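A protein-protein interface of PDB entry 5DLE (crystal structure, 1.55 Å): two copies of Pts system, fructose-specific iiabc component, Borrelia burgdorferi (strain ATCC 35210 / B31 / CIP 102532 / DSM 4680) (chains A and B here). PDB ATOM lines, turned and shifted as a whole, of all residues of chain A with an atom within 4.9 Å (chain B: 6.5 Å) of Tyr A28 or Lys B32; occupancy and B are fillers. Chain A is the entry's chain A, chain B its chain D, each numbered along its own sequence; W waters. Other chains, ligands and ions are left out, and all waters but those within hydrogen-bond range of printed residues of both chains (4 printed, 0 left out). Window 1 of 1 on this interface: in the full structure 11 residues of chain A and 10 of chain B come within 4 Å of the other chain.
Water W4 bridges the side-chain amide nitrogen of Asn B36 (2.5 Å) and the side-chain hydroxyl of Tyr A28 (3.4 Å). Water W3 lies within hydrogen-bond range of NZ of Lys A32, OE1 of Glu A35 and OE1 of Glu B35. Water W2 lies within hydrogen-bond range of the side-chain amino group of Lys A32 (2.7 Å), the backbone carbonyl oxygen of Val B47 (2.7 Å) and the side-chain carboxylate of Glu B35 (3.3 Å). Water W1 lies within hydrogen-bond range of the side-chain carboxylate of Glu B35 (2.7 Å), the side-chain amino group of Lys B32 (3.0 Å) and the side-chain carboxylate of Glu A35 (3.2 Å).
Printed residues of chain B within 4 Å of Val A24: Ile B29 (3.6 Å). Of the printed residues of chain B, Ala A25 touches Ala B25 (3.8 Å). Of the printed residues of chain A, Ile B29 touches Val A24 (3.6 Å) and Tyr A28 (3.5 Å). Lys B32 touches just these residues of chain A: Tyr A28, Ala A31, Lys A32 and Glu A35. Asn B36 touches none of the printed residues of chain A. The nearest residue of chain B that does not touch Tyr A28 is Tyr B28 (4.4 Å).
Ala A25 touches its own counterpart, Ala B25. Ile A29 touches Ala B25, but with the chains exchanged Ala A25 does not touch Ile B29 (4.5 Å). Ala A31 touches Lys B32, but with the chains exchanged Lys A32 does not touch Ala B31 (4.3 Å). Lys A32 touches Glu B35, and with the chains exchanged Glu A35 touches Lys B32. Positions printed for both chains: 18, 25, 27, 28, 29, 30, 31, 32, 33 and 35. Of the 13 pairs that touch across the chains among the printed residues, 8 have their exchanged pair printed and touching as well.
Among the printed residues, pairs that only touch across the chains: Val A24 with Ile B29 (3.6 Å), Ala A25 with Ala B25 (3.8 Å), Tyr A28 with Ile B29 (3.5 Å), Tyr A28 with Lys B32 (3.8 Å), Ile A29 with Ala B25 (3.97 Å), Ala A31 with Lys B32 (3.8 Å), Lys A32 with Tyr B28 (3.5 Å), Lys A32 with Lys B32 (3.9 Å) and Lys A33 with Tyr B28 (3.8 Å).
NZ of Lys B32 lies within salt-bridge range of OE2 of Glu A35, 2.7 Å away. The side-chain amino group of Lys A32 lies within salt-bridge range of the side-chain carboxylate of Glu B35, 2.7 Å away. The side-chain carboxylate (OE2) of Glu A56 is in salt-bridge range of the side-chain amino group (NZ) of Lys B33 (2.7 Å). The side-chain hydroxyl (OH) of Tyr A28 sits at hydrogen-bond distance from the side-chain amino group (NZ) of Lys B33, 3.1 Å away.
Printed residues of chain B that touch a printed residue of chain A: Ala B25, Tyr B28, Ile B29, Lys B32, Lys B33 and Glu B35. Hydrophobic or aromatic side chains of chain B within 4 Å of the printed part of chain A: Ala B25, Tyr B28 and Ile B29. Printed residues of chain A that touch a printed residue of chain B: Val A24, Ala A25, Tyr A28, Ile A29, Ala A31, Lys A32, Lys A33, Glu A35 and Glu A56. Among the printed residues, Asp or Glu carboxylates within 4 Å of a Lys or Arg side-chain nitrogen of the other chain: Lys A32 with Glu B35 (2.7 Å), Glu A35 with Lys B32 (2.7 Å) and Glu A56 with Lys B33 (2.7 Å).
The backbone carbonyl oxygen (O) of Lys B32 lies within hydrogen-bond range of the side-chain amide nitrogen (ND2) of Asn B36 (3.2 Å). The side-chain hydroxyl (OH) of Tyr A28 lies close to the side-chain carboxylate (OE2) of Glu A56, at 3.4 Å. N of Glu A56 is in hydrogen-bond range of O of Thr A49 (2.8 Å).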
ATOM      1  N   THR A  18     -17.412   6.381   1.688  1.00  0.00           N
ATOM      2  CA  THR A  18     -17.334   6.837   3.067  1.00  0.00           C
ATOM      3  C   THR A  18     -16.015   7.580   3.216  1.00  0.00           C
ATOM      4  O   THR A  18     -14.982   7.168   2.673  1.00  0.00           O
ATOM      5  CB  THR A  18     -17.469   5.714   4.065  1.00  0.00           C
ATOM      6  OG1 THR A  18     -16.313   4.843   4.019  1.00  0.00           O
ATOM      7  CG2 THR A  18     -18.791   4.934   3.820  1.00  0.00           C
ATOM      8  N   VAL A  24      -9.036   6.098  10.766  1.00  0.00           N
ATOM      9  CA  VAL A  24      -9.744   5.177   9.864  1.00  0.00           C
ATOM     10  C   VAL A  24     -11.073   4.700  10.412  1.00  0.00           C
ATOM     11  O   VAL A  24     -11.869   4.103   9.651  1.00  0.00           O
ATOM     12  CB  VAL A  24      -8.889   3.944   9.518  1.00  0.00           C
ATOM     13  CG1 VAL A  24      -7.700   4.378   8.623  1.00  0.00           C
ATOM     14  CG2 VAL A  24      -8.438   3.163  10.782  1.00  0.00           C
ATOM     15  N   ALA A  25     -11.382   4.956  11.687  1.00  0.00           N
ATOM     16  CA  ALA A  25     -12.514   4.271  12.320  1.00  0.00           C
ATOM     17  C   ALA A  25     -13.858   4.666  11.682  1.00  0.00           C
ATOM     18  O   ALA A  25     -14.647   3.793  11.274  1.00  0.00           O
ATOM     19  CB  ALA A  25     -12.590   4.529  13.823  1.00  0.00           C
ATOM     20  N   HIS A  26     -14.191   5.957  11.648  1.00  0.00           N
ATOM     21  CA  HIS A  26     -15.499   6.306  11.074  1.00  0.00           C
ATOM     22  C   HIS A  26     -15.617   5.876   9.622  1.00  0.00           C
ATOM     23  O   HIS A  26     -16.699   5.433   9.196  1.00  0.00           O
ATOM     24  CB  HIS A  26     -15.821   7.787  11.188  1.00  0.00           C
ATOM     25  CG  HIS A  26     -16.298   8.171  12.553  1.00  0.00           C
ATOM     26  ND1 HIS A  26     -17.175   9.213  12.750  1.00  0.00           N
ATOM     27  CD2 HIS A  26     -15.976   7.703  13.782  1.00  0.00           C
ATOM     28  CE1 HIS A  26     -17.380   9.371  14.058  1.00  0.00           C
ATOM     29  NE2 HIS A  26     -16.668   8.468  14.705  1.00  0.00           N
ATOM     30  N   THR A  27     -14.539   6.024   8.846  1.00  0.00           N
ATOM     31  CA  THR A  27     -14.577   5.589   7.435  1.00  0.00           C
ATOM     32  C   THR A  27     -14.973   4.127   7.342  1.00  0.00           C
ATOM     33  O   THR A  27     -15.868   3.761   6.536  1.00  0.00           O
ATOM     34  CB  THR A  27     -13.199   5.792   6.824  1.00  0.00           C
ATOM     35  OG1 THR A  27     -12.934   7.190   6.797  1.00  0.00           O
ATOM     36  CG2 THR A  27     -13.106   5.240   5.420  1.00  0.00           C
ATOM     37  N   TYR A  28     -14.326   3.279   8.146  1.00  0.00           N
ATOM     38  CA  TYR A  28     -14.559   1.839   8.024  1.00  0.00           C
ATOM     39  C   TYR A  28     -15.823   1.416   8.744  1.00  0.00           C
ATOM     40  O   TYR A  28     -16.498   0.466   8.303  1.00  0.00           O
ATOM     41  CB  TYR A  28     -13.341   1.041   8.574  1.00  0.00           C
ATOM     42  CG  TYR A  28     -12.281   0.862   7.502  1.00  0.00           C
ATOM     43  CD1 TYR A  28     -11.406   1.863   7.190  1.00  0.00           C
ATOM     44  CD2 TYR A  28     -12.232  -0.303   6.751  1.00  0.00           C
ATOM     45  CE1 TYR A  28     -10.472   1.741   6.183  1.00  0.00           C
ATOM     46  CE2 TYR A  28     -11.330  -0.437   5.737  1.00  0.00           C
ATOM     47  CZ  TYR A  28     -10.456   0.577   5.458  1.00  0.00           C
ATOM     48  OH  TYR A  28      -9.532   0.437   4.441  1.00  0.00           O
ATOM     49  N   ILE A  29     -16.164   2.053   9.880  1.00  0.00           N
ATOM     50  CA  ILE A  29     -17.416   1.666  10.524  1.00  0.00           C
ATOM     51  C   ILE A  29     -18.590   2.000   9.596  1.00  0.00           C
ATOM     52  O   ILE A  29     -19.516   1.197   9.431  1.00  0.00           O
ATOM     53  CB  ILE A  29     -17.572   2.366  11.889  1.00  0.00           C
ATOM     54  CG1 ILE A  29     -16.497   1.849  12.858  1.00  0.00           C
ATOM     55  CG2 ILE A  29     -18.948   2.016  12.495  1.00  0.00           C
ATOM     56  CD1 ILE A  29     -16.374   2.748  14.114  1.00  0.00           C
ATOM     57  N   ALA A  30     -18.600   3.230   9.037  1.00  0.00           N
ATOM     58  CA  ALA A  30     -19.679   3.592   8.128  1.00  0.00           C
ATOM     59  C   ALA A  30     -19.741   2.619   6.959  1.00  0.00           C
ATOM     60  O   ALA A  30     -20.839   2.166   6.572  1.00  0.00           O
ATOM     61  CB  ALA A  30     -19.508   5.028   7.628  1.00  0.00           C
ATOM     62  N   ALA A  31     -18.576   2.238   6.429  1.00  0.00           N
ATOM     63  CA  ALA A  31     -18.590   1.347   5.257  1.00  0.00           C
ATOM     64  C   ALA A  31     -19.161  -0.002   5.599  1.00  0.00           C
ATOM     65  O   ALA A  31     -20.014  -0.532   4.861  1.00  0.00           O
ATOM     66  CB  ALA A  31     -17.182   1.193   4.690  1.00  0.00           C
ATOM     67  N   LYS A  32     -18.715  -0.567   6.728  1.00  0.00           N
ATOM     68  CA  LYS A  32     -19.130  -1.914   7.070  1.00  0.00           C
ATOM     69  C   LYS A  32     -20.588  -1.925   7.489  1.00  0.00           C
ATOM     70  O   LYS A  32     -21.325  -2.864   7.155  1.00  0.00           O
ATOM     71  CB  LYS A  32     -18.213  -2.486   8.139  1.00  0.00           C
ATOM     72  CG  LYS A  32     -18.417  -3.935   8.448  1.00  0.00           C
ATOM     73  CD  LYS A  32     -18.247  -4.873   7.211  1.00  0.00           C
ATOM     74  CE  LYS A  32     -18.539  -6.254   7.696  1.00  0.00           C
ATOM     75  NZ  LYS A  32     -18.690  -7.219   6.577  1.00  0.00           N
ATOM     76  N   LYS A  33     -21.063  -0.891   8.182  1.00  0.00           N
ATOM     77  CA  LYS A  33     -22.485  -0.880   8.527  1.00  0.00           C
ATOM     78  C   LYS A  33     -23.341  -0.714   7.285  1.00  0.00           C
ATOM     79  O   LYS A  33     -24.406  -1.346   7.178  1.00  0.00           O
ATOM     80  CB  LYS A  33     -22.804   0.207   9.545  1.00  0.00           C
ATOM     81  CG  LYS A  33     -22.146  -0.105  10.863  1.00  0.00           C
ATOM     82  CD  LYS A  33     -22.663   0.751  11.961  1.00  0.00           C
ATOM     83  CE  LYS A  33     -23.948   0.178  12.570  1.00  0.00           C
ATOM     84  NZ  LYS A  33     -24.165   0.941  13.856  1.00  0.00           N
ATOM     85  N   GLU A  35     -22.526  -1.733   4.236  1.00  0.00           N
ATOM     86  CA  GLU A  35     -22.467  -3.049   3.564  1.00  0.00           C
ATOM     87  C   GLU A  35     -23.396  -4.053   4.235  1.00  0.00           C
ATOM     88  O   GLU A  35     -24.138  -4.753   3.546  1.00  0.00           O
ATOM     89  CB  GLU A  35     -21.029  -3.567   3.560  1.00  0.00           C
ATOM     90  CG  GLU A  35     -20.117  -2.785   2.626  1.00  0.00           C
ATOM     91  CD  GLU A  35     -18.624  -3.020   2.857  1.00  0.00           C
ATOM     92  OE1 GLU A  35     -18.243  -3.823   3.758  1.00  0.00           O
ATOM     93  OE2 GLU A  35     -17.831  -2.365   2.143  1.00  0.00           O
ATOM     94  N   THR A  49     -13.594   3.854   0.113  1.00  0.00           N
ATOM     95  CA  THR A  49     -13.281   4.469   1.391  1.00  0.00           C
ATOM     96  C   THR A  49     -12.186   5.518   1.240  1.00  0.00           C
ATOM     97  O   THR A  49     -11.278   5.371   0.428  1.00  0.00           O
ATOM     98  CB  THR A  49     -12.823   3.425   2.443  1.00  0.00           C
ATOM     99  OG1 THR A  49     -11.723   2.645   1.948  1.00  0.00           O
ATOM    100  CG2 THR A  49     -13.967   2.484   2.842  1.00  0.00           C
ATOM    101  N   GLU A  56      -9.218   4.053  -1.021  1.00  0.00           N
ATOM    102  CA  GLU A  56      -9.122   2.619  -1.281  1.00  0.00           C
ATOM    103  C   GLU A  56     -10.386   2.161  -2.000  1.00  0.00           C
ATOM    104  O   GLU A  56     -11.478   2.657  -1.726  1.00  0.00           O
ATOM    105  CB  GLU A  56      -8.948   1.808   0.017  1.00  0.00           C
ATOM    106  CG  GLU A  56      -7.619   2.031   0.725  1.00  0.00           C
ATOM    107  CD  GLU A  56      -7.613   1.377   2.108  1.00  0.00           C
ATOM    108  OE1 GLU A  56      -8.353   1.859   3.007  1.00  0.00           O
ATOM    109  OE2 GLU A  56      -6.903   0.360   2.279  1.00  0.00           O
ATOM    110  N   THR B  18     -13.559 -11.821  13.198  1.00  0.00           N
ATOM    111  CA  THR B  18     -12.806 -10.708  13.765  1.00  0.00           C
ATOM    112  C   THR B  18     -13.464 -10.321  15.073  1.00  0.00           C
ATOM    113  O   THR B  18     -14.699 -10.333  15.181  1.00  0.00           O
ATOM    114  CB  THR B  18     -12.743  -9.499  12.822  1.00  0.00           C
ATOM    115  OG1 THR B  18     -14.043  -8.887  12.631  1.00  0.00           O
ATOM    116  CG2 THR B  18     -12.130  -9.885  11.443  1.00  0.00           C
ATOM    117  N   ALA B  25     -14.661  -0.590  15.967  1.00  0.00           N
ATOM    118  CA  ALA B  25     -13.762  -0.167  14.905  1.00  0.00           C
ATOM    119  C   ALA B  25     -12.814  -1.274  14.465  1.00  0.00           C
ATOM    120  O   ALA B  25     -12.762  -1.604  13.281  1.00  0.00           O
ATOM    121  CB  ALA B  25     -12.977   1.056  15.358  1.00  0.00           C
ATOM    122  N   THR B  27     -12.848  -4.391  14.936  1.00  0.00           N
ATOM    123  CA  THR B  27     -13.593  -5.542  14.406  1.00  0.00           C
ATOM    124  C   THR B  27     -13.970  -5.306  12.946  1.00  0.00           C
ATOM    125  O   THR B  27     -13.789  -6.193  12.087  1.00  0.00           O
ATOM    126  CB  THR B  27     -14.849  -5.748  15.251  1.00  0.00           C
ATOM    127  OG1 THR B  27     -14.453  -6.205  16.538  1.00  0.00           O
ATOM    128  CG2 THR B  27     -15.819  -6.772  14.589  1.00  0.00           C
ATOM    129  N   TYR B  28     -14.495  -4.112  12.638  1.00  0.00           N
ATOM    130  CA  TYR B  28     -14.963  -3.838  11.283  1.00  0.00           C
ATOM    131  C   TYR B  28     -13.834  -3.540  10.327  1.00  0.00           C
ATOM    132  O   TYR B  28     -13.901  -3.919   9.145  1.00  0.00           O
ATOM    133  CB  TYR B  28     -15.960  -2.663  11.328  1.00  0.00           C
ATOM    134  CG  TYR B  28     -17.351  -2.969  11.862  1.00  0.00           C
ATOM    135  CD1 TYR B  28     -17.867  -4.251  11.922  1.00  0.00           C
ATOM    136  CD2 TYR B  28     -18.186  -1.918  12.211  1.00  0.00           C
ATOM    137  CE1 TYR B  28     -19.205  -4.480  12.315  1.00  0.00           C
ATOM    138  CE2 TYR B  28     -19.491  -2.130  12.626  1.00  0.00           C
ATOM    139  CZ  TYR B  28     -19.999  -3.397  12.658  1.00  0.00           C
ATOM    140  OH  TYR B  28     -21.317  -3.566  13.044  1.00  0.00           O
ATOM    141  N   ILE B  29     -12.768  -2.859  10.803  1.00  0.00           N
ATOM    142  CA  ILE B  29     -11.631  -2.595   9.930  1.00  0.00           C
ATOM    143  C   ILE B  29     -10.972  -3.915   9.544  1.00  0.00           C
ATOM    144  O   ILE B  29     -10.741  -4.170   8.366  1.00  0.00           O
ATOM    145  CB  ILE B  29     -10.612  -1.653  10.611  1.00  0.00           C
ATOM    146  CG1 ILE B  29     -11.211  -0.307  10.930  1.00  0.00           C
ATOM    147  CG2 ILE B  29      -9.410  -1.459   9.678  1.00  0.00           C
ATOM    148  CD1 ILE B  29     -10.299   0.391  12.060  1.00  0.00           C
ATOM    149  N   ALA B  30     -10.718  -4.788  10.534  1.00  0.00           N
ATOM    150  CA  ALA B  30     -10.137  -6.089  10.207  1.00  0.00           C
ATOM    151  C   ALA B  30     -11.030  -6.861   9.256  1.00  0.00           C
ATOM    152  O   ALA B  30     -10.516  -7.500   8.317  1.00  0.00           O
ATOM    153  CB  ALA B  30      -9.871  -6.896  11.479  1.00  0.00           C
ATOM    154  N   ALA B  31     -12.355  -6.817   9.487  1.00  0.00           N
ATOM    155  CA  ALA B  31     -13.251  -7.580   8.601  1.00  0.00           C
ATOM    156  C   ALA B  31     -13.155  -7.080   7.175  1.00  0.00           C
ATOM    157  O   ALA B  31     -13.062  -7.887   6.241  1.00  0.00           O
ATOM    158  CB  ALA B  31     -14.694  -7.501   9.102  1.00  0.00           C
ATOM    159  N   LYS B  32     -13.202  -5.752   6.972  1.00  0.00           N
ATOM    160  CA  LYS B  32     -13.142  -5.233   5.606  1.00  0.00           C
ATOM    161  C   LYS B  32     -11.785  -5.511   4.971  1.00  0.00           C
ATOM    162  O   LYS B  32     -11.705  -5.841   3.783  1.00  0.00           O
ATOM    163  CB  LYS B  32     -13.431  -3.724   5.575  1.00  0.00           C
ATOM    164  CG  LYS B  32     -14.923  -3.474   5.655  1.00  0.00           C
ATOM    165  CD  LYS B  32     -15.319  -2.029   5.244  1.00  0.00           C
ATOM    166  CE  LYS B  32     -14.707  -1.572   3.919  1.00  0.00           C
ATOM    167  NZ  LYS B  32     -15.208  -2.379   2.747  1.00  0.00           N
ATOM    168  N   LYS B  33     -10.704  -5.393   5.736  1.00  0.00           N
ATOM    169  CA  LYS B  33      -9.382  -5.650   5.158  1.00  0.00           C
ATOM    170  C   LYS B  33      -9.257  -7.106   4.733  1.00  0.00           C
ATOM    171  O   LYS B  33      -8.743  -7.408   3.647  1.00  0.00           O
ATOM    172  CB  LYS B  33      -8.277  -5.302   6.173  1.00  0.00           C
ATOM    173  CG  LYS B  33      -8.130  -3.820   6.513  1.00  0.00           C
ATOM    174  CD  LYS B  33      -7.462  -3.052   5.438  1.00  0.00           C
ATOM    175  CE  LYS B  33      -7.204  -1.619   5.922  1.00  0.00           C
ATOM    176  NZ  LYS B  33      -6.739  -0.791   4.767  1.00  0.00           N
ATOM    177  N   ILE B  34      -9.742  -8.025   5.567  1.00  0.00           N
ATOM    178  CA  ILE B  34      -9.682  -9.446   5.217  1.00  0.00           C
ATOM    179  C   ILE B  34     -10.559  -9.722   4.003  1.00  0.00           C
ATOM    180  O   ILE B  34     -10.145 -10.446   3.082  1.00  0.00           O
ATOM    181  CB  ILE B  34     -10.101 -10.283   6.441  1.00  0.00           C
ATOM    182  CG1 ILE B  34      -8.982 -10.271   7.471  1.00  0.00           C
ATOM    183  CG2 ILE B  34     -10.443 -11.737   6.013  1.00  0.00           C
ATOM    184  CD1 ILE B  34      -9.384 -10.810   8.832  1.00  0.00           C
ATOM    185  N   GLU B  35     -11.784  -9.180   3.989  1.00  0.00           N
ATOM    186  CA  GLU B  35     -12.703  -9.398   2.850  1.00  0.00           C
ATOM    187  C   GLU B  35     -12.068  -8.918   1.553  1.00  0.00           C
ATOM    188  O   GLU B  35     -12.066  -9.634   0.538  1.00  0.00           O
ATOM    189  CB  GLU B  35     -14.033  -8.659   3.088  1.00  0.00           C
ATOM    190  CG  GLU B  35     -14.963  -9.320   4.112  1.00  0.00           C
ATOM    191  CD  GLU B  35     -16.008  -8.396   4.785  1.00  0.00           C
ATOM    192  OE1 GLU B  35     -16.088  -7.177   4.492  1.00  0.00           O
ATOM    193  OE2 GLU B  35     -16.761  -8.914   5.645  1.00  0.00           O
ATOM    194  N   ASN B  36     -11.544  -7.698   1.552  1.00  0.00           N
ATOM    195  CA  ASN B  36     -11.005  -7.169   0.302  1.00  0.00           C
ATOM    196  C   ASN B  36      -9.765  -7.956  -0.136  1.00  0.00           C
ATOM    197  O   ASN B  36      -9.619  -8.264  -1.328  1.00  0.00           O
ATOM    198  CB  ASN B  36     -10.722  -5.664   0.458  1.00  0.00           C
ATOM    199  CG  ASN B  36     -12.009  -4.819   0.448  1.00  0.00           C
ATOM    200  OD1 ASN B  36     -12.919  -5.048  -0.364  1.00  0.00           O
ATOM    201  ND2 ASN B  36     -12.088  -3.832   1.352  1.00  0.00           N
ATOM    202  N   GLU B  37      -8.888  -8.320   0.798  1.00  0.00           N
ATOM    203  CA  GLU B  37      -7.658  -9.002   0.408  1.00  0.00           C
ATOM    204  C   GLU B  37      -7.914 -10.453  -0.015  1.00  0.00           C
ATOM    205  O   GLU B  37      -7.245 -10.946  -0.930  1.00  0.00           O
ATOM    206  CB  GLU B  37      -6.617  -8.949   1.531  1.00  0.00           C
ATOM    207  CG  GLU B  37      -5.291  -9.605   1.181  1.00  0.00           C
ATOM    208  CD  GLU B  37      -4.522  -8.865   0.081  1.00  0.00           C
ATOM    209  OE1 GLU B  37      -4.673  -7.656  -0.081  1.00  0.00           O
ATOM    210  OE2 GLU B  37      -3.747  -9.552  -0.629  1.00  0.00           O
ATOM    211  N   VAL B  47     -16.910 -13.530   6.704  1.00  0.00           N
ATOM    212  CA  VAL B  47     -16.368 -12.994   7.958  1.00  0.00           C
ATOM    213  C   VAL B  47     -17.511 -12.784   8.956  1.00  0.00           C
ATOM    214  O   VAL B  47     -18.449 -12.003   8.708  1.00  0.00           O
ATOM    215  CB  VAL B  47     -15.579 -11.678   7.773  1.00  0.00           C
ATOM    216  CG1 VAL B  47     -14.953 -11.310   9.117  1.00  0.00           C
ATOM    217  CG2 VAL B  47     -14.496 -11.890   6.691  1.00  0.00           C
HETATM  218  O   HOH W   1     -15.630  -5.321   2.584  1.00  0.00           O
HETATM  219  O   HOH W   2     -18.983  -9.485   7.967  1.00  0.00           O
HETATM  220  O   HOH W   3     -19.015  -6.457   4.188  1.00  0.00           O
HETATM  221  O   HOH W   4     -10.920  -2.132   2.779  1.00  0.00           O
